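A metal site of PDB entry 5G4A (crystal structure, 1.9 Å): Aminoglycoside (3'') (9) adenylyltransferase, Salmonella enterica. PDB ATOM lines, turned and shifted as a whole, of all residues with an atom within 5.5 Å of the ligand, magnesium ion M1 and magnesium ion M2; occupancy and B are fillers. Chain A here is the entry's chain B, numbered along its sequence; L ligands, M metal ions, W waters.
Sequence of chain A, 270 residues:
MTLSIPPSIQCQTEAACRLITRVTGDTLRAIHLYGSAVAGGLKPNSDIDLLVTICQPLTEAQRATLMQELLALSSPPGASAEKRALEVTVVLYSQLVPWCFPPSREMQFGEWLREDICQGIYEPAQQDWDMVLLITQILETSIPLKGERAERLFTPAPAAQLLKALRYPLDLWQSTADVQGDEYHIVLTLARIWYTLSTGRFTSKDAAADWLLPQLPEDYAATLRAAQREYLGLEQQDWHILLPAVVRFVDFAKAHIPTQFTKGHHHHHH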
ATOM      1  N   TYR A  34      15.432   0.333  -0.253  1.00  0.00           N
ATOM      2  CA  TYR A  34      14.252   0.367  -1.112  1.00  0.00           C
ATOM      3  C   TYR A  34      13.055  -0.106  -0.289  1.00  0.00           C
ATOM      4  O   TYR A  34      13.138  -0.224   0.937  1.00  0.00           O
ATOM      5  CB  TYR A  34      14.513  -0.476  -2.367  1.00  0.00           C
ATOM      6  CG  TYR A  34      14.546  -1.972  -2.077  1.00  0.00           C
ATOM      7  CD1 TYR A  34      15.698  -2.598  -1.560  1.00  0.00           C
ATOM      8  CD2 TYR A  34      13.430  -2.757  -2.327  1.00  0.00           C
ATOM      9  CE1 TYR A  34      15.718  -3.981  -1.311  1.00  0.00           C
ATOM     10  CE2 TYR A  34      13.426  -4.134  -2.043  1.00  0.00           C
ATOM     11  CZ  TYR A  34      14.568  -4.739  -1.565  1.00  0.00           C
ATOM     12  OH  TYR A  34      14.537  -6.096  -1.307  1.00  0.00           O
ATOM     13  N   GLY A  35      11.929  -0.384  -0.964  1.00  0.00           N
ATOM     14  CA  GLY A  35      10.800  -0.940  -0.220  1.00  0.00           C
ATOM     15  C   GLY A  35      10.078   0.143   0.565  1.00  0.00           C
ATOM     16  O   GLY A  35      10.237   1.343   0.304  1.00  0.00           O
ATOM     17  N   SER A  36       9.262  -0.271   1.533  1.00  0.00           N
ATOM     18  CA  SER A  36       8.264   0.646   2.069  1.00  0.00           C
ATOM     19  C   SER A  36       8.898   1.805   2.853  1.00  0.00           C
ATOM     20  O   SER A  36       8.268   2.859   2.975  1.00  0.00           O
ATOM     21  CB  SER A  36       7.238  -0.100   2.932  1.00  0.00           C
ATOM     22  OG  SER A  36       7.793  -0.557   4.164  1.00  0.00           O
ATOM     23  N   ALA A  37      10.111   1.628   3.392  1.00  0.00           N
ATOM     24  CA  ALA A  37      10.777   2.737   4.055  1.00  0.00           C
ATOM     25  C   ALA A  37      10.983   3.904   3.103  1.00  0.00           C
ATOM     26  O   ALA A  37      11.020   5.063   3.539  1.00  0.00           O
ATOM     27  CB  ALA A  37      12.126   2.291   4.611  1.00  0.00           C
ATOM     28  N   GLY A  40       6.935   4.144   0.743  1.00  0.00           N
ATOM     29  CA  GLY A  40       5.715   4.445   1.460  1.00  0.00           C
ATOM     30  C   GLY A  40       5.100   3.210   2.075  1.00  0.00           C
ATOM     31  O   GLY A  40       5.212   2.085   1.560  1.00  0.00           O
ATOM     32  N   GLY A  41       4.430   3.409   3.208  1.00  0.00           N
ATOM     33  CA  GLY A  41       3.752   2.333   3.903  1.00  0.00           C
ATOM     34  C   GLY A  41       4.609   1.657   4.956  1.00  0.00           C
ATOM     35  O   GLY A  41       4.542   0.438   5.119  1.00  0.00           O
ATOM     36  N   LEU A  42       5.398   2.432   5.683  1.00  0.00           N
ATOM     37  CA  LEU A  42       6.221   1.866   6.752  1.00  0.00           C
ATOM     38  C   LEU A  42       5.346   1.665   7.985  1.00  0.00           C
ATOM     39  O   LEU A  42       4.947   2.630   8.638  1.00  0.00           O
ATOM     40  CB  LEU A  42       7.400   2.789   7.063  1.00  0.00           C
ATOM     41  CG  LEU A  42       8.388   2.247   8.091  1.00  0.00           C
ATOM     42  CD1 LEU A  42       9.239   1.189   7.430  1.00  0.00           C
ATOM     43  CD2 LEU A  42       9.237   3.379   8.577  1.00  0.00           C
ATOM     44  N   LYS A  43       5.064   0.402   8.308  1.00  0.00           N
ATOM     45  CA  LYS A  43       4.204   0.001   9.411  1.00  0.00           C
ATOM     46  C   LYS A  43       5.041  -0.519  10.587  1.00  0.00           C
ATOM     47  O   LYS A  43       6.226  -0.815  10.436  1.00  0.00           O
ATOM     48  CB  LYS A  43       3.244  -1.097   8.935  1.00  0.00           C
ATOM     49  CG  LYS A  43       2.442  -0.709   7.695  1.00  0.00           C
ATOM     50  CD  LYS A  43       1.602   0.512   8.027  1.00  0.00           C
ATOM     51  CE  LYS A  43       0.752   0.927   6.862  1.00  0.00           C
ATOM     52  NZ  LYS A  43      -0.263   1.933   7.275  1.00  0.00           N
ATOM     53  N   SER A  46       6.925  -3.488   9.764  1.00  0.00           N
ATOM     54  CA  SER A  46       7.642  -3.454   8.489  1.00  0.00           C
ATOM     55  C   SER A  46       9.138  -3.638   8.704  1.00  0.00           C
ATOM     56  O   SER A  46       9.709  -3.243   9.737  1.00  0.00           O
ATOM     57  CB  SER A  46       7.365  -2.140   7.759  1.00  0.00           C
ATOM     58  OG  SER A  46       6.036  -2.111   7.269  1.00  0.00           O
ATOM     59  N   ASP A  47       9.762  -4.275   7.727  1.00  0.00           N
ATOM     60  CA  ASP A  47      11.198  -4.458   7.713  1.00  0.00           C
ATOM     61  C   ASP A  47      11.883  -3.265   7.055  1.00  0.00           C
ATOM     62  O   ASP A  47      11.236  -2.349   6.540  1.00  0.00           O
ATOM     63  CB  ASP A  47      11.544  -5.778   7.015  1.00  0.00           C
ATOM     64  CG  ASP A  47      11.080  -5.818   5.539  1.00  0.00           C
ATOM     65  OD1 ASP A  47      10.605  -4.816   4.980  1.00  0.00           O
ATOM     66  OD2 ASP A  47      11.212  -6.902   4.924  1.00  0.00           O
ATOM     67  N   ILE A  48      13.217  -3.284   7.034  1.00  0.00           N
ATOM     68  CA  ILE A  48      14.050  -2.351   6.291  1.00  0.00           C
ATOM     69  C   ILE A  48      14.698  -3.141   5.161  1.00  0.00           C
ATOM     70  O   ILE A  48      15.442  -4.094   5.422  1.00  0.00           O
ATOM     71  CB  ILE A  48      15.131  -1.698   7.167  1.00  0.00           C
ATOM     72  CG1 ILE A  48      14.535  -0.865   8.303  1.00  0.00           C
ATOM     73  CG2 ILE A  48      16.092  -0.834   6.270  1.00  0.00           C
ATOM     74  CD1 ILE A  48      15.543  -0.454   9.394  1.00  0.00           C
ATOM     75  N   ASP A  49      14.440  -2.757   3.911  1.00  0.00           N
ATOM     76  CA  ASP A  49      14.850  -3.555   2.756  1.00  0.00           C
ATOM     77  C   ASP A  49      16.122  -2.991   2.145  1.00  0.00           C
ATOM     78  O   ASP A  49      16.153  -1.818   1.747  1.00  0.00           O
ATOM     79  CB  ASP A  49      13.764  -3.606   1.688  1.00  0.00           C
ATOM     80  CG  ASP A  49      12.509  -4.318   2.152  1.00  0.00           C
ATOM     81  OD1 ASP A  49      12.561  -5.547   2.345  1.00  0.00           O
ATOM     82  OD2 ASP A  49      11.460  -3.650   2.294  1.00  0.00           O
ATOM     83  N   GLU A  87      16.101  -6.911   6.060  1.00  0.00           N
ATOM     84  CA  GLU A  87      16.222  -7.868   4.977  1.00  0.00           C
ATOM     85  C   GLU A  87      17.359  -7.399   4.083  1.00  0.00           C
ATOM     86  O   GLU A  87      17.296  -6.297   3.533  1.00  0.00           O
ATOM     87  CB  GLU A  87      14.936  -8.010   4.164  1.00  0.00           C
ATOM     88  CG  GLU A  87      15.091  -9.046   3.059  1.00  0.00           C
ATOM     89  CD  GLU A  87      13.844  -9.214   2.207  1.00  0.00           C
ATOM     90  OE1 GLU A  87      12.763  -8.775   2.627  1.00  0.00           O
ATOM     91  OE2 GLU A  87      13.961  -9.809   1.112  1.00  0.00           O
ATOM     92  N   ASP A 130      12.368 -13.291  -8.110  1.00  0.00           N
ATOM     93  CA  ASP A 130      12.014 -12.039  -7.436  1.00  0.00           C
ATOM     94  C   ASP A 130      13.085 -10.976  -7.601  1.00  0.00           C
ATOM     95  O   ASP A 130      12.779  -9.788  -7.533  1.00  0.00           O
ATOM     96  CB  ASP A 130      11.726 -12.275  -5.950  1.00  0.00           C
ATOM     97  CG  ASP A 130      11.083 -11.053  -5.305  1.00  0.00           C
ATOM     98  OD1 ASP A 130      10.027 -10.599  -5.814  1.00  0.00           O
ATOM     99  OD2 ASP A 130      11.656 -10.532  -4.323  1.00  0.00           O
ATOM    100  N   LEU A 133      12.051  -8.368  -9.901  1.00  0.00           N
ATOM    101  CA  LEU A 133      11.147  -7.398  -9.310  1.00  0.00           C
ATOM    102  C   LEU A 133      11.902  -6.435  -8.385  1.00  0.00           C
ATOM    103  O   LEU A 133      11.609  -5.230  -8.378  1.00  0.00           O
ATOM    104  CB  LEU A 133      10.037  -8.119  -8.544  1.00  0.00           C
ATOM    105  CG  LEU A 133       9.201  -9.198  -9.269  1.00  0.00           C
ATOM    106  CD1 LEU A 133       8.031  -9.609  -8.399  1.00  0.00           C
ATOM    107  CD2 LEU A 133       8.675  -8.764 -10.611  1.00  0.00           C
ATOM    108  N   LEU A 134      12.858  -6.936  -7.601  1.00  0.00           N
ATOM    109  CA  LEU A 134      13.632  -6.070  -6.717  1.00  0.00           C
ATOM    110  C   LEU A 134      14.320  -4.955  -7.491  1.00  0.00           C
ATOM    111  O   LEU A 134      14.150  -3.768  -7.166  1.00  0.00           O
ATOM    112  CB  LEU A 134      14.666  -6.895  -5.934  1.00  0.00           C
ATOM    113  CG  LEU A 134      14.068  -7.890  -4.938  1.00  0.00           C
ATOM    114  CD1 LEU A 134      15.150  -8.414  -3.986  1.00  0.00           C
ATOM    115  CD2 LEU A 134      12.898  -7.285  -4.159  1.00  0.00           C
ATOM    116  N   GLN A 137      11.881  -2.450  -8.937  1.00  0.00           N
ATOM    117  CA  GLN A 137      11.401  -1.524  -7.904  1.00  0.00           C
ATOM    118  C   GLN A 137      12.480  -0.534  -7.503  1.00  0.00           C
ATOM    119  O   GLN A 137      12.190   0.648  -7.291  1.00  0.00           O
ATOM    120  CB  GLN A 137      10.911  -2.296  -6.689  1.00  0.00           C
ATOM    121  CG  GLN A 137       9.554  -2.875  -6.908  1.00  0.00           C
ATOM    122  CD  GLN A 137       9.155  -3.820  -5.829  1.00  0.00           C
ATOM    123  OE1 GLN A 137       8.609  -3.418  -4.804  1.00  0.00           O
ATOM    124  NE2 GLN A 137       9.423  -5.095  -6.046  1.00  0.00           N
ATOM    125  N   LEU A 166       6.707 -11.503 -12.531  1.00  0.00           N
ATOM    126  CA  LEU A 166       5.487 -11.126 -11.834  1.00  0.00           C
ATOM    127  C   LEU A 166       4.538 -12.311 -11.685  1.00  0.00           C
ATOM    128  O   LEU A 166       3.890 -12.468 -10.648  1.00  0.00           O
ATOM    129  CB  LEU A 166       4.771 -10.002 -12.585  1.00  0.00           C
ATOM    130  CG  LEU A 166       5.333  -8.611 -12.351  1.00  0.00           C
ATOM    131  CD1 LEU A 166       4.795  -7.694 -13.440  1.00  0.00           C
ATOM    132  CD2 LEU A 166       4.922  -8.124 -10.911  1.00  0.00           C
ATOM    133  N   HIS A 185      -0.598 -12.203   3.709  1.00  0.00           N
ATOM    134  CA  HIS A 185       0.498 -11.763   2.856  1.00  0.00           C
ATOM    135  C   HIS A 185       0.250 -12.179   1.409  1.00  0.00           C
ATOM    136  O   HIS A 185       0.460 -11.384   0.479  1.00  0.00           O
ATOM    137  CB  HIS A 185       1.831 -12.312   3.359  1.00  0.00           C
ATOM    138  CG  HIS A 185       3.002 -11.985   2.468  1.00  0.00           C
ATOM    139  ND1 HIS A 185       3.362 -10.691   2.153  1.00  0.00           N
ATOM    140  CD2 HIS A 185       3.891 -12.784   1.840  1.00  0.00           C
ATOM    141  CE1 HIS A 185       4.419 -10.707   1.366  1.00  0.00           C
ATOM    142  NE2 HIS A 185       4.766 -11.962   1.166  1.00  0.00           N
ATOM    143  N   THR A 189      -0.066  -9.721  -1.732  1.00  0.00           N
ATOM    144  CA  THR A 189       0.914  -9.796  -2.817  1.00  0.00           C
ATOM    145  C   THR A 189       0.213  -9.977  -4.165  1.00  0.00           C
ATOM    146  O   THR A 189       0.625  -9.378  -5.170  1.00  0.00           O
ATOM    147  CB  THR A 189       1.884 -10.931  -2.554  1.00  0.00           C
ATOM    148  OG1 THR A 189       2.544 -10.690  -1.301  1.00  0.00           O
ATOM    149  CG2 THR A 189       2.944 -11.045  -3.690  1.00  0.00           C
ATOM    150  N   ARG A 192      -0.901  -6.702  -5.303  1.00  0.00           N
ATOM    151  CA  ARG A 192       0.176  -5.924  -5.906  1.00  0.00           C
ATOM    152  C   ARG A 192       0.554  -6.452  -7.288  1.00  0.00           C
ATOM    153  O   ARG A 192       0.879  -5.676  -8.187  1.00  0.00           O
ATOM    154  CB  ARG A 192       1.433  -5.893  -5.031  1.00  0.00           C
ATOM    155  CG  ARG A 192       1.214  -5.328  -3.628  1.00  0.00           C
ATOM    156  CD  ARG A 192       2.527  -5.375  -2.846  1.00  0.00           C
ATOM    157  NE  ARG A 192       3.318  -4.160  -3.014  1.00  0.00           N
ATOM    158  CZ  ARG A 192       4.489  -3.963  -2.411  1.00  0.00           C
ATOM    159  NH1 ARG A 192       4.993  -4.919  -1.637  1.00  0.00           N
ATOM    160  NH2 ARG A 192       5.159  -2.836  -2.591  1.00  0.00           N
ATOM    161  N   ILE A 193       0.557  -7.776  -7.452  1.00  0.00           N
ATOM    162  CA  ILE A 193       0.883  -8.335  -8.771  1.00  0.00           C
ATOM    163  C   ILE A 193      -0.153  -7.889  -9.782  1.00  0.00           C
ATOM    164  O   ILE A 193       0.185  -7.477 -10.904  1.00  0.00           O
ATOM    165  CB  ILE A 193       0.980  -9.879  -8.696  1.00  0.00           C
ATOM    166  CG1 ILE A 193       2.287 -10.295  -8.030  1.00  0.00           C
ATOM    167  CG2 ILE A 193       0.887 -10.502 -10.101  1.00  0.00           C
ATOM    168  CD1 ILE A 193       2.274 -11.761  -7.573  1.00  0.00           C
ATOM    169  N   THR A 196       0.375  -4.169 -10.643  1.00  0.00           N
ATOM    170  CA  THR A 196       1.520  -3.938 -11.510  1.00  0.00           C
ATOM    171  C   THR A 196       1.248  -4.385 -12.945  1.00  0.00           C
ATOM    172  O   THR A 196       1.645  -3.713 -13.905  1.00  0.00           O
ATOM    173  CB  THR A 196       2.756  -4.646 -10.965  1.00  0.00           C
ATOM    174  OG1 THR A 196       3.034  -4.142  -9.640  1.00  0.00           O
ATOM    175  CG2 THR A 196       3.962  -4.362 -11.870  1.00  0.00           C
ATOM    176  N   PHE A 202       4.397   0.144  -9.544  1.00  0.00           N
ATOM    177  CA  PHE A 202       4.468  -0.499  -8.241  1.00  0.00           C
ATOM    178  C   PHE A 202       3.802   0.387  -7.192  1.00  0.00           C
ATOM    179  O   PHE A 202       3.846   1.620  -7.279  1.00  0.00           O
ATOM    180  CB  PHE A 202       5.924  -0.801  -7.847  1.00  0.00           C
ATOM    181  CG  PHE A 202       6.560  -1.803  -8.739  1.00  0.00           C
ATOM    182  CD1 PHE A 202       6.424  -3.162  -8.472  1.00  0.00           C
ATOM    183  CD2 PHE A 202       7.202  -1.404  -9.897  1.00  0.00           C
ATOM    184  CE1 PHE A 202       6.970  -4.100  -9.324  1.00  0.00           C
ATOM    185  CE2 PHE A 202       7.755  -2.344 -10.742  1.00  0.00           C
ATOM    186  CZ  PHE A 202       7.641  -3.689 -10.463  1.00  0.00           C
ATOM    187  N   THR A 203       3.160  -0.249  -6.215  1.00  0.00           N
ATOM    188  CA  THR A 203       2.460   0.513  -5.195  1.00  0.00           C
ATOM    189  C   THR A 203       2.461  -0.291  -3.913  1.00  0.00           C
ATOM    190  O   THR A 203       2.766  -1.489  -3.914  1.00  0.00           O
ATOM    191  CB  THR A 203       1.022   0.873  -5.656  1.00  0.00           C
ATOM    192  OG1 THR A 203       0.503   1.963  -4.895  1.00  0.00           O
ATOM    193  CG2 THR A 203       0.112  -0.327  -5.490  1.00  0.00           C
ATOM    194  N   SER A 204       2.123   0.370  -2.813  1.00  0.00           N
ATOM    195  CA  SER A 204       2.187  -0.255  -1.498  1.00  0.00           C
ATOM    196  C   SER A 204       1.125  -1.351  -1.364  1.00  0.00           C
ATOM    197  O   SER A 204       0.142  -1.398  -2.117  1.00  0.00           O
ATOM    198  CB  SER A 204       1.974   0.776  -0.385  1.00  0.00           C
ATOM    199  OG  SER A 204       0.666   1.334  -0.451  1.00  0.00           O
ATOM    200  N   LYS A 205       1.337  -2.224  -0.373  1.00  0.00           N
ATOM    201  CA  LYS A 205       0.362  -3.282  -0.102  1.00  0.00           C
ATOM    202  C   LYS A 205      -1.028  -2.697   0.136  1.00  0.00           C
ATOM    203  O   LYS A 205      -2.018  -3.217  -0.369  1.00  0.00           O
ATOM    204  CB  LYS A 205       0.825  -4.110   1.087  1.00  0.00           C
ATOM    205  CG  LYS A 205       1.983  -5.041   0.731  1.00  0.00           C
ATOM    206  CD  LYS A 205       2.754  -5.491   1.982  1.00  0.00           C
ATOM    207  CE  LYS A 205       3.957  -6.386   1.584  1.00  0.00           C
ATOM    208  NZ  LYS A 205       4.608  -6.932   2.844  1.00  0.00           N
ATOM    209  N   TYR A 231      -3.305  -6.537   8.036  1.00  0.00           N
ATOM    210  CA  TYR A 231      -1.994  -5.957   7.746  1.00  0.00           C
ATOM    211  C   TYR A 231      -1.881  -4.568   8.350  1.00  0.00           C
ATOM    212  O   TYR A 231      -0.826  -4.201   8.881  1.00  0.00           O
ATOM    213  CB  TYR A 231      -1.760  -5.912   6.244  1.00  0.00           C
ATOM    214  CG  TYR A 231      -0.444  -5.268   5.885  1.00  0.00           C
ATOM    215  CD1 TYR A 231       0.743  -5.988   5.973  1.00  0.00           C
ATOM    216  CD2 TYR A 231      -0.382  -3.950   5.497  1.00  0.00           C
ATOM    217  CE1 TYR A 231       1.954  -5.407   5.662  1.00  0.00           C
ATOM    218  CE2 TYR A 231       0.826  -3.356   5.190  1.00  0.00           C
ATOM    219  CZ  TYR A 231       1.985  -4.086   5.273  1.00  0.00           C
ATOM    220  OH  TYR A 231       3.183  -3.465   4.956  1.00  0.00           O
HETATM  221  P1  LIG L   1       6.456  -3.892   4.260  1.00  0.00           P
HETATM  222  O1  LIG L   1       6.325  -2.544   4.901  1.00  0.00           O
HETATM  223  O2  LIG L   1       7.871  -4.527   4.389  1.00  0.00           O
HETATM  224  O3  LIG L   1       5.400  -4.873   4.740  1.00  0.00           O
HETATM  225  P2  LIG L   1       7.146  -3.706   1.466  1.00  0.00           P
HETATM  226  O4  LIG L   1       8.484  -3.206   1.829  1.00  0.00           O
HETATM  227  O5  LIG L   1       6.563  -2.973   0.302  1.00  0.00           O
HETATM  228  O6  LIG L   1       6.148  -3.672   2.716  1.00  0.00           O
HETATM  229  P3  LIG L   1       8.219  -6.419   1.509  1.00  0.00           P
HETATM  230  O7  LIG L   1       9.404  -5.893   2.277  1.00  0.00           O
HETATM  231  O8  LIG L   1       7.440  -7.428   2.293  1.00  0.00           O
HETATM  232  O9  LIG L   1       7.243  -5.248   1.046  1.00  0.00           O
HETATM  233  O10 LIG L   1       8.676  -7.043   0.128  1.00  0.00           O
HETATM  234  C1  LIG L   1       7.658  -7.326  -0.841  1.00  0.00           C
HETATM  235  C2  LIG L   1       8.073  -8.539  -1.638  1.00  0.00           C
HETATM  236  O11 LIG L   1       7.013  -8.850  -2.566  1.00  0.00           O
HETATM  237  C3  LIG L   1       9.333  -8.328  -2.487  1.00  0.00           C
HETATM  238  O12 LIG L   1      10.082  -9.547  -2.553  1.00  0.00           O
HETATM  239  C4  LIG L   1       8.733  -7.950  -3.848  1.00  0.00           C
HETATM  240  O13 LIG L   1       9.615  -8.116  -4.953  1.00  0.00           O
HETATM  241  C5  LIG L   1       7.543  -8.897  -3.875  1.00  0.00           C
HETATM  242  N1  LIG L   1       6.498  -8.573  -4.829  1.00  0.00           N
HETATM  243  C6  LIG L   1       5.885  -9.459  -5.682  1.00  0.00           C
HETATM  244  N2  LIG L   1       5.092  -8.899  -6.564  1.00  0.00           N
HETATM  245  C7  LIG L   1       5.172  -7.544  -6.248  1.00  0.00           C
HETATM  246  C8  LIG L   1       4.576  -6.406  -6.830  1.00  0.00           C
HETATM  247  N3  LIG L   1       3.793  -6.453  -7.915  1.00  0.00           N
HETATM  248  N4  LIG L   1       4.852  -5.210  -6.280  1.00  0.00           N
HETATM  249  C9  LIG L   1       5.673  -5.154  -5.226  1.00  0.00           C
HETATM  250  N5  LIG L   1       6.308  -6.157  -4.603  1.00  0.00           N
HETATM  251  C10 LIG L   1       6.012  -7.334  -5.171  1.00  0.00           C
HETATM  252 MG    MG M   1      11.280  -7.248   2.794  1.00  0.00          MG
HETATM  253 MG    MG M   2       9.636  -4.104   3.363  1.00  0.00          MG
HETATM  254  O   HOH W   1      12.122  -6.731  -0.260  1.00  0.00           O
HETATM  255  O   HOH W   2       4.050  -1.819   0.800  1.00  0.00           O
HETATM  256  O   HOH W   3      10.306  -4.395  -0.446  1.00  0.00           O
HETATM  257  O   HOH W   4       2.951  -3.194  -6.783  1.00  0.00           O
HETATM  258  O   HOH W   5       4.651  -4.505   7.926  1.00  0.00           O
HETATM  259  O   HOH W   6       3.489  -1.329   3.360  1.00  0.00           O
HETATM  260  O   HOH W   7       9.876  -2.254   4.430  1.00  0.00           O
HETATM  261  O   HOH W   8       7.997  -6.907   5.902  1.00  0.00           O
HETATM  262  O   HOH W   9       4.467  -7.820  -1.708  1.00  0.00           O
HETATM  263  O   HOH W  10       9.722  -9.023   2.993  1.00  0.00           O
HETATM  264  O   HOH W  11       8.921 -12.183  -2.242  1.00  0.00           O
HETATM  265  O   HOH W  12       8.030  -4.214  -2.313  1.00  0.00           O
HETATM  266  O   HOH W  13       7.656  -1.106  -1.339  1.00  0.00           O
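Water W13 lies within hydrogen-bond range of O5 of the ligand (2.7 Å), NH2 of Arg 192 (3.3 Å) and N of Ser 36 (3.4 Å).
Water W9 lies within hydrogen-bond range of an oxygen (O11) of the ligand (2.9 Å), the guanidinium group of Arg 192 (2.9 Å) and the side-chain hydroxyl of Thr 189 (3.5 Å).
Water W1 lies within hydrogen-bond range of the side-chain hydroxyl of Tyr 34 and an oxygen (O10) of the ligand.
Water W12 lies within hydrogen-bond range of the side-chain amide oxygen (OE1) of Gln 137 (2.7 Å), the guanidinium group (NH1) of Arg 192 (3.2 Å) and an oxygen (O5) of the ligand (3.2 Å).
Water W5 lies within hydrogen-bond range of the side-chain hydroxyl of Ser 46, an oxygen (O3) of the ligand and the side-chain hydroxyl of Tyr 231.
Water W6 lies within hydrogen-bond range of OH of Tyr 231 (2.7 Å), O of Gly 41 (2.7 Å) and O1 of the ligand (3.4 Å).
A nitrogen (N3) of the ligand sits at hydrogen-bond distance from the backbone carbonyl oxygen of Arg 192.
An oxygen (O5) of the ligand is in salt-bridge range of the guanidinium group (NH1) of Arg 192 (3.2 Å).
The side-chain amide nitrogen of Gln 137 sits at hydrogen-bond distance from an oxygen (O13) of the ligand, 3.2 Å away.
O3 of the ligand lies within hydrogen-bond range of OH of Tyr 231.
N of Ser 36 lies close to O4 of the ligand.
The side-chain amino group (NZ) of Lys 205 is in salt-bridge range of an oxygen (O3) of the ligand (2.9 Å).
The side-chain carboxylate of Asp 130 sits at hydrogen-bond distance from an oxygen (O12) of the ligand, at 2.6 Å.
OG of Ser 46 lies within hydrogen-bond range of O1 of the ligand.
The side-chain hydroxyl (OG) of Ser 36 lies within hydrogen-bond range of an oxygen (O1) of the ligand.
N3 of the ligand sits at hydrogen-bond distance from OG1 of Thr 196, at 3.0 Å.
An oxygen (O1) of the ligand lies close to the backbone carbonyl oxygen (O) of Gly 41 (3.5 Å).
Merely in contact with the ligand: Gly 35 (3.8 Å), Leu 133 (3.5 Å), Leu 134 (3.5 Å), Leu 166 (3.6 Å), Thr 189 (3.9 Å), Ile 193 (3.5 Å) and Phe 202 (3.4 Å).
The nearest printed residue that does not touch the ligand is Glu 87 (4.4 Å).
Magnesium ion M1 is bound by OE1 of Glu 87, OD2 of Asp 47, OD1 of Asp 49, water W10 and O7 of the ligand.
Magnesium ion M1 has five donor atoms within binding distance.
Of the 28 residues printed, 3 come within 4 Å of magnesium ion M1.
Along chain A the residues within 4 Å of magnesium ion M1 span positions 47 to 87.
The nearest printed residue that does not touch magnesium ion M1 is Tyr 34 (5.4 Å).
Two residues have an atom within 4 Å of magnesium ion M2: Asp 47 and Asp 49.
The nearest printed residue that does not touch magnesium ion M2 is Ser 36 (4.1 Å).
Magnesium ion M2 is bound by OD1 of Asp 47 (2.0 Å), O2 of the ligand (2.1 Å), O7 of the ligand (2.1 Å), O4 of the ligand (2.1 Å), water W7 (2.1 Å) and OD2 of Asp 49 (2.2 Å).
Magnesium ion M2 has six donor atoms within binding distance.
The backbone carbonyl oxygen (O) of Arg 192 is in hydrogen-bond range of the side-chain hydroxyl (OG1) of Thr 196.
The side-chain hydroxyl (OG1) of Thr 189 sits at hydrogen-bond distance from the backbone carbonyl oxygen (O) of His 185 (2.8 Å).
The guanidinium group (NE) of Arg 192 lies within hydrogen-bond range of the backbone carbonyl oxygen (O) of Thr 203 (2.9 Å).
NE2 of Gln 137 lies within hydrogen-bond range of O of Leu 133 (3.2 Å).
The side-chain hydroxyl (OG) of Ser 46 sits at hydrogen-bond distance from the backbone NH (N) of Lys 43 (2.9 Å).
N of Tyr 34 lies within hydrogen-bond range of O of Asp 49 (3.0 Å).
The backbone NH (N) of Glu 87 lies within hydrogen-bond range of the backbone carbonyl oxygen (O) of Ile 48 (3.0 Å).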
